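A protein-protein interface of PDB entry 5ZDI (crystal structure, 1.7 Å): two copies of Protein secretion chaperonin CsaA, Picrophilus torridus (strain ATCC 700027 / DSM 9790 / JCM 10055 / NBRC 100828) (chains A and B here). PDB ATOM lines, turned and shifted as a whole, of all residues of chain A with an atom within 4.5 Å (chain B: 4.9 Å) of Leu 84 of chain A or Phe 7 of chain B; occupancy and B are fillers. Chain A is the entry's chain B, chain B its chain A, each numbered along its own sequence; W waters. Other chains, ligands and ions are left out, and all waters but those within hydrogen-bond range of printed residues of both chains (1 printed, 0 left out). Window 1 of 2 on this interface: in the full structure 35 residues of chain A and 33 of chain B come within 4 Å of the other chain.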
ATOM      1  N   ILE A  10     -20.436 -22.880 -18.159  1.00  0.00           N
ATOM      2  CA  ILE A  10     -19.014 -22.859 -18.449  1.00  0.00           C
ATOM      3  C   ILE A  10     -18.783 -21.515 -19.213  1.00  0.00           C
ATOM      4  O   ILE A  10     -19.481 -21.213 -20.162  1.00  0.00           O
ATOM      5  CB  ILE A  10     -18.569 -24.026 -19.392  1.00  0.00           C
ATOM      6  CG1 ILE A  10     -19.092 -25.435 -18.980  1.00  0.00           C
ATOM      7  CG2 ILE A  10     -17.059 -24.041 -19.483  1.00  0.00           C
ATOM      8  CD1 ILE A  10     -18.603 -25.937 -17.683  1.00  0.00           C
ATOM      9  N   ILE A  12     -16.542 -19.622 -21.585  1.00  0.00           N
ATOM     10  CA  ILE A  12     -15.542 -19.878 -22.616  1.00  0.00           C
ATOM     11  C   ILE A  12     -15.282 -18.575 -23.375  1.00  0.00           C
ATOM     12  O   ILE A  12     -16.250 -17.945 -23.866  1.00  0.00           O
ATOM     13  CB  ILE A  12     -16.020 -20.967 -23.558  1.00  0.00           C
ATOM     14  CG1 ILE A  12     -16.355 -22.211 -22.753  1.00  0.00           C
ATOM     15  CG2 ILE A  12     -14.953 -21.235 -24.632  1.00  0.00           C
ATOM     16  CD1 ILE A  12     -16.834 -23.361 -23.572  1.00  0.00           C
ATOM     17  N   ILE A  64      -8.994 -20.220 -27.516  1.00  0.00           N
ATOM     18  CA  ILE A  64     -10.220 -20.315 -26.837  1.00  0.00           C
ATOM     19  C   ILE A  64      -9.966 -20.975 -25.518  1.00  0.00           C
ATOM     20  O   ILE A  64      -9.333 -22.022 -25.462  1.00  0.00           O
ATOM     21  CB  ILE A  64     -11.208 -21.216 -27.678  1.00  0.00           C
ATOM     22  CG1 ILE A  64     -11.399 -20.654 -29.101  1.00  0.00           C
ATOM     23  CG2 ILE A  64     -12.553 -21.371 -27.005  1.00  0.00           C
ATOM     24  CD1 ILE A  64     -11.862 -19.213 -29.161  1.00  0.00           C
ATOM     25  N   VAL A  66     -11.583 -21.976 -21.259  1.00  0.00           N
ATOM     26  CA  VAL A  66     -12.506 -21.895 -20.129  1.00  0.00           C
ATOM     27  C   VAL A  66     -11.886 -21.048 -19.037  1.00  0.00           C
ATOM     28  O   VAL A  66     -10.730 -21.308 -18.606  1.00  0.00           O
ATOM     29  CB  VAL A  66     -12.769 -23.270 -19.532  1.00  0.00           C
ATOM     30  CG1 VAL A  66     -13.680 -23.097 -18.338  1.00  0.00           C
ATOM     31  CG2 VAL A  66     -13.324 -24.254 -20.587  1.00  0.00           C
ATOM     32  N   PHE A  69     -12.862 -21.959 -14.254  1.00  0.00           N
ATOM     33  CA  PHE A  69     -12.412 -23.073 -13.397  1.00  0.00           C
ATOM     34  C   PHE A  69     -11.736 -22.504 -12.165  1.00  0.00           C
ATOM     35  O   PHE A  69     -11.151 -21.405 -12.217  1.00  0.00           O
ATOM     36  CB  PHE A  69     -11.356 -23.933 -14.104  1.00  0.00           C
ATOM     37  CG  PHE A  69     -11.892 -24.815 -15.182  1.00  0.00           C
ATOM     38  CD1 PHE A  69     -12.947 -25.647 -14.944  1.00  0.00           C
ATOM     39  CD2 PHE A  69     -11.242 -24.910 -16.384  1.00  0.00           C
ATOM     40  CE1 PHE A  69     -13.401 -26.514 -15.907  1.00  0.00           C
ATOM     41  CE2 PHE A  69     -11.671 -25.783 -17.330  1.00  0.00           C
ATOM     42  CZ  PHE A  69     -12.738 -26.599 -17.117  1.00  0.00           C
ATOM     43  N   LEU A  82      -8.083 -23.193 -18.946  1.00  0.00           N
ATOM     44  CA  LEU A  82      -7.929 -24.370 -19.805  1.00  0.00           C
ATOM     45  C   LEU A  82      -8.017 -23.892 -21.264  1.00  0.00           C
ATOM     46  O   LEU A  82      -9.082 -23.466 -21.693  1.00  0.00           O
ATOM     47  CB  LEU A  82      -8.986 -25.428 -19.511  1.00  0.00           C
ATOM     48  CG  LEU A  82      -8.878 -26.665 -20.461  1.00  0.00           C
ATOM     49  CD1 LEU A  82      -7.555 -27.438 -20.281  1.00  0.00           C
ATOM     50  CD2 LEU A  82     -10.144 -27.497 -20.363  1.00  0.00           C
ATOM     51  N   VAL A  83      -6.970 -24.105 -22.018  1.00  0.00           N
ATOM     52  CA  VAL A  83      -6.944 -23.728 -23.417  1.00  0.00           C
ATOM     53  C   VAL A  83      -7.484 -24.928 -24.190  1.00  0.00           C
ATOM     54  O   VAL A  83      -7.118 -26.078 -23.899  1.00  0.00           O
ATOM     55  CB  VAL A  83      -5.521 -23.421 -23.868  1.00  0.00           C
ATOM     56  CG1 VAL A  83      -5.466 -23.205 -25.383  1.00  0.00           C
ATOM     57  CG2 VAL A  83      -5.011 -22.211 -23.142  1.00  0.00           C
ATOM     58  N   LEU A  84      -8.330 -24.692 -25.168  1.00  0.00           N
ATOM     59  CA  LEU A  84      -9.079 -25.810 -25.784  1.00  0.00           C
ATOM     60  C   LEU A  84      -8.413 -26.247 -27.052  1.00  0.00           C
ATOM     61  O   LEU A  84      -8.028 -25.457 -27.911  1.00  0.00           O
ATOM     62  CB  LEU A  84     -10.507 -25.382 -26.099  1.00  0.00           C
ATOM     63  CG  LEU A  84     -11.355 -25.135 -24.791  1.00  0.00           C
ATOM     64  CD1 LEU A  84     -12.763 -24.890 -25.340  1.00  0.00           C
ATOM     65  CD2 LEU A  84     -11.254 -26.198 -23.672  1.00  0.00           C
ATOM     66  N   GLY A  85      -8.278 -27.551 -27.169  1.00  0.00           N
ATOM     67  CA  GLY A  85      -7.782 -28.114 -28.407  1.00  0.00           C
ATOM     68  C   GLY A  85      -8.323 -29.515 -28.638  1.00  0.00           C
ATOM     69  O   GLY A  85      -8.769 -30.163 -27.668  1.00  0.00           O
ATOM     70  N   LEU A  94      -5.002 -26.761 -31.471  1.00  0.00           N
ATOM     71  CA  LEU A  94      -5.766 -25.628 -30.910  1.00  0.00           C
ATOM     72  C   LEU A  94      -7.001 -25.226 -31.753  1.00  0.00           C
ATOM     73  O   LEU A  94      -6.974 -25.143 -32.992  1.00  0.00           O
ATOM     74  CB  LEU A  94      -4.899 -24.395 -30.656  1.00  0.00           C
ATOM     75  CG  LEU A  94      -3.759 -24.588 -29.699  1.00  0.00           C
ATOM     76  CD1 LEU A  94      -2.883 -23.385 -29.779  1.00  0.00           C
ATOM     77  CD2 LEU A  94      -4.236 -24.872 -28.274  1.00  0.00           C
ATOM     78  N   LEU A  95      -7.981 -24.826 -30.999  1.00  0.00           N
ATOM     79  CA  LEU A  95      -9.095 -24.117 -31.480  1.00  0.00           C
ATOM     80  C   LEU A  95      -8.741 -22.636 -31.598  1.00  0.00           C
ATOM     81  O   LEU A  95      -8.075 -22.061 -30.685  1.00  0.00           O
ATOM     82  CB  LEU A  95     -10.313 -24.266 -30.565  1.00  0.00           C
ATOM     83  CG  LEU A  95     -10.784 -25.610 -30.125  1.00  0.00           C
ATOM     84  CD1 LEU A  95     -12.229 -25.537 -29.619  1.00  0.00           C
ATOM     85  CD2 LEU A  95     -10.728 -26.629 -31.203  1.00  0.00           C
ATOM     86  N   THR B   3     -16.521 -27.008 -11.772  1.00  0.00           N
ATOM     87  CA  THR B   3     -15.319 -27.927 -11.705  1.00  0.00           C
ATOM     88  C   THR B   3     -14.698 -28.339 -13.004  1.00  0.00           C
ATOM     89  O   THR B   3     -15.386 -28.314 -13.998  1.00  0.00           O
ATOM     90  CB  THR B   3     -15.728 -29.201 -10.938  1.00  0.00           C
ATOM     91  OG1 THR B   3     -16.913 -29.814 -11.511  1.00  0.00           O
ATOM     92  CG2 THR B   3     -16.023 -28.811  -9.509  1.00  0.00           C
ATOM     93  N   TYR B   4     -13.440 -28.866 -13.018  1.00  0.00           N
ATOM     94  CA  TYR B   4     -12.850 -29.517 -14.257  1.00  0.00           C
ATOM     95  C   TYR B   4     -13.721 -30.679 -14.654  1.00  0.00           C
ATOM     96  O   TYR B   4     -13.934 -30.928 -15.904  1.00  0.00           O
ATOM     97  CB  TYR B   4     -11.327 -29.935 -14.189  1.00  0.00           C
ATOM     98  CG  TYR B   4     -10.313 -28.830 -14.610  1.00  0.00           C
ATOM     99  CD1 TYR B   4      -9.921 -27.809 -13.713  1.00  0.00           C
ATOM    100  CD2 TYR B   4      -9.732 -28.800 -15.876  1.00  0.00           C
ATOM    101  CE1 TYR B   4      -9.008 -26.800 -14.077  1.00  0.00           C
ATOM    102  CE2 TYR B   4      -8.823 -27.775 -16.240  1.00  0.00           C
ATOM    103  CZ  TYR B   4      -8.468 -26.760 -15.358  1.00  0.00           C
ATOM    104  OH  TYR B   4      -7.552 -25.703 -15.750  1.00  0.00           O
ATOM    105  N   ASN B   5     -14.317 -31.317 -13.632  1.00  0.00           N
ATOM    106  CA  ASN B   5     -15.298 -32.364 -13.912  1.00  0.00           C
ATOM    107  C   ASN B   5     -16.539 -31.880 -14.657  1.00  0.00           C
ATOM    108  O   ASN B   5     -17.057 -32.615 -15.537  1.00  0.00           O
ATOM    109  CB  ASN B   5     -15.736 -33.099 -12.646  1.00  0.00           C
ATOM    110  CG  ASN B   5     -16.145 -34.515 -12.933  1.00  0.00           C
ATOM    111  OD1 ASN B   5     -17.332 -34.825 -12.943  1.00  0.00           O
ATOM    112  ND2 ASN B   5     -15.162 -35.362 -13.285  1.00  0.00           N
ATOM    113  N   ASP B   6     -17.057 -30.690 -14.302  1.00  0.00           N
ATOM    114  CA  ASP B   6     -18.193 -30.136 -15.000  1.00  0.00           C
ATOM    115  C   ASP B   6     -17.927 -30.010 -16.509  1.00  0.00           C
ATOM    116  O   ASP B   6     -18.801 -30.275 -17.311  1.00  0.00           O
ATOM    117  CB  ASP B   6     -18.639 -28.789 -14.466  1.00  0.00           C
ATOM    118  CG  ASP B   6     -19.303 -28.873 -13.076  1.00  0.00           C
ATOM    119  OD1 ASP B   6     -19.814 -29.979 -12.708  1.00  0.00           O
ATOM    120  OD2 ASP B   6     -19.273 -27.813 -12.376  1.00  0.00           O
ATOM    121  N   PHE B   7     -16.721 -29.636 -16.895  1.00  0.00           N
ATOM    122  CA  PHE B   7     -16.429 -29.471 -18.313  1.00  0.00           C
ATOM    123  C   PHE B   7     -16.350 -30.832 -19.004  1.00  0.00           C
ATOM    124  O   PHE B   7     -16.848 -31.006 -20.095  1.00  0.00           O
ATOM    125  CB  PHE B   7     -15.130 -28.706 -18.463  1.00  0.00           C
ATOM    126  CG  PHE B   7     -14.770 -28.438 -19.894  1.00  0.00           C
ATOM    127  CD1 PHE B   7     -15.567 -27.625 -20.645  1.00  0.00           C
ATOM    128  CD2 PHE B   7     -13.683 -29.069 -20.484  1.00  0.00           C
ATOM    129  CE1 PHE B   7     -15.225 -27.372 -21.962  1.00  0.00           C
ATOM    130  CE2 PHE B   7     -13.366 -28.845 -21.821  1.00  0.00           C
ATOM    131  CZ  PHE B   7     -14.156 -28.004 -22.549  1.00  0.00           C
ATOM    132  N   SER B   8     -15.800 -31.830 -18.320  1.00  0.00           N
ATOM    133  CA  SER B   8     -15.659 -33.179 -18.888  1.00  0.00           C
ATOM    134  C   SER B   8     -17.000 -33.796 -19.238  1.00  0.00           C
ATOM    135  O   SER B   8     -17.037 -34.665 -20.092  1.00  0.00           O
ATOM    136  CB  SER B   8     -14.835 -34.126 -17.951  1.00  0.00           C
ATOM    137  OG  SER B   8     -15.566 -34.552 -16.821  1.00  0.00           O
ATOM    138  N   LYS B   9     -18.098 -33.342 -18.585  1.00  0.00           N
ATOM    139  CA  LYS B   9     -19.455 -33.831 -18.862  1.00  0.00           C
ATOM    140  C   LYS B   9     -19.886 -33.480 -20.328  1.00  0.00           C
ATOM    141  O   LYS B   9     -20.782 -34.137 -20.894  1.00  0.00           O
ATOM    142  CB  LYS B   9     -20.532 -33.218 -17.942  1.00  0.00           C
ATOM    143  CG  LYS B   9     -20.466 -33.490 -16.422  1.00  0.00           C
ATOM    144  CD  LYS B   9     -21.503 -32.630 -15.690  1.00  0.00           C
ATOM    145  CE  LYS B   9     -21.359 -32.696 -14.162  1.00  0.00           C
ATOM    146  NZ  LYS B   9     -22.426 -31.868 -13.534  1.00  0.00           N
ATOM    147  N   ILE B  10     -19.338 -32.375 -20.837  1.00  0.00           N
ATOM    148  CA  ILE B  10     -19.682 -31.897 -22.182  1.00  0.00           C
ATOM    149  C   ILE B  10     -18.824 -32.621 -23.254  1.00  0.00           C
ATOM    150  O   ILE B  10     -17.616 -32.699 -23.162  1.00  0.00           O
ATOM    151  CB  ILE B  10     -19.488 -30.358 -22.369  1.00  0.00           C
ATOM    152  CG1 ILE B  10     -19.880 -29.532 -21.131  1.00  0.00           C
ATOM    153  CG2 ILE B  10     -20.296 -29.896 -23.599  1.00  0.00           C
ATOM    154  CD1 ILE B  10     -21.303 -29.652 -20.714  1.00  0.00           C
ATOM    155  N   ILE B  12     -17.499 -32.468 -26.711  1.00  0.00           N
ATOM    156  CA  ILE B  12     -17.252 -31.460 -27.773  1.00  0.00           C
ATOM    157  C   ILE B  12     -16.410 -32.122 -28.846  1.00  0.00           C
ATOM    158  O   ILE B  12     -15.321 -32.708 -28.530  1.00  0.00           O
ATOM    159  CB  ILE B  12     -16.619 -30.198 -27.238  1.00  0.00           C
ATOM    160  CG1 ILE B  12     -17.444 -29.661 -26.062  1.00  0.00           C
ATOM    161  CG2 ILE B  12     -16.426 -29.188 -28.365  1.00  0.00           C
ATOM    162  CD1 ILE B  12     -16.818 -28.472 -25.359  1.00  0.00           C
ATOM    163  N   ILE B 106     -12.481 -32.744 -28.119  1.00  0.00           N
ATOM    164  CA  ILE B 106     -11.787 -31.647 -27.473  1.00  0.00           C
ATOM    165  C   ILE B 106     -11.377 -32.091 -26.061  1.00  0.00           C
ATOM    166  O   ILE B 106     -12.181 -32.624 -25.324  1.00  0.00           O
ATOM    167  CB  ILE B 106     -12.650 -30.324 -27.464  1.00  0.00           C
ATOM    168  CG1 ILE B 106     -12.521 -29.594 -28.822  1.00  0.00           C
ATOM    169  CG2 ILE B 106     -12.211 -29.414 -26.297  1.00  0.00           C
ATOM    170  CD1 ILE B 106     -12.766 -30.387 -30.099  1.00  0.00           C
ATOM    171  N   ALA B 107     -10.120 -31.825 -25.673  1.00  0.00           N
ATOM    172  CA  ALA B 107      -9.504 -32.338 -24.429  1.00  0.00           C
ATOM    173  C   ALA B 107     -10.058 -31.636 -23.217  1.00  0.00           C
ATOM    174  O   ALA B 107     -10.324 -30.429 -23.281  1.00  0.00           O
ATOM    175  CB  ALA B 107      -7.991 -32.126 -24.463  1.00  0.00           C
ATOM    176  OXT ALA B 107     -10.200 -32.267 -22.123  1.00  0.00           O
HETATM  177  O   HOH W   1      -8.509 -28.692 -24.627  1.00  0.00           O
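The backbone NH (N) of Ala 107 of chain B lies within hydrogen-bond range of the backbone carbonyl oxygen (O) of Gly 85 of chain A (2.9 Å).
Water W1 lies within hydrogen-bond range of N of Gly 85 of chain A (2.8 Å), O of Ala 107 of chain B (2.9 Å) and O of Val 83 of chain A (3.0 Å).
Among the printed residues, pairs that only touch across the chains: Phe 69 of chain A with Thr 3 of chain B (3.3 Å), Gly 85 of chain A with Ile 106 of chain B (3.4 Å), Phe 69 of chain A with Phe 7 of chain B (3.5 Å), Phe 69 of chain A with Tyr 4 of chain B (3.5 Å), Leu 84 of chain A with Phe 7 of chain B (3.6 Å), Leu 82 of chain A with Phe 7 of chain B (3.8 Å) and Val 66 of chain A with Phe 7 of chain B (3.9 Å).
The backbone carbonyl oxygen of Leu 84 of chain A lies within hydrogen-bond range of the backbone NH of Leu 95 of chain A, 3.2 Å away.
The backbone carbonyl oxygen (O) of Ile 64 of chain A is in hydrogen-bond range of the backbone NH (N) of Leu 84 of chain A.
The side-chain hydroxyl (OG1) of Thr 3 of chain B lies within hydrogen-bond range of the backbone NH (N) of Asp 6 of chain B, 2.9 Å away.
The backbone carbonyl oxygen of Leu 82 of chain A sits at hydrogen-bond distance from the backbone NH of Val 66 of chain A, 2.9 Å away.
The backbone carbonyl oxygen (O) of Ile 12 of chain B is in hydrogen-bond range of the backbone NH (N) of Ile 106 of chain B, at 2.9 Å.
Leu 84 of chain A touches just one residue of chain B: Phe 7 (3.6 Å).
Of the printed residues of chain B, Gly 85 of chain A touches Ile 106 and Ala 107.
Printed residues of chain A within 4 Å of Phe 7 of chain B: Val 66, Phe 69, Leu 82 and Leu 84.
Of the printed residues of chain A, Ile 106 of chain B touches Gly 85 (3.4 Å).
Positions printed for both chains: 10 and 12.
Among the printed residues, no Asp or Glu carboxylate lies within 4 Å of a Lys or Arg side-chain nitrogen of the other chain.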
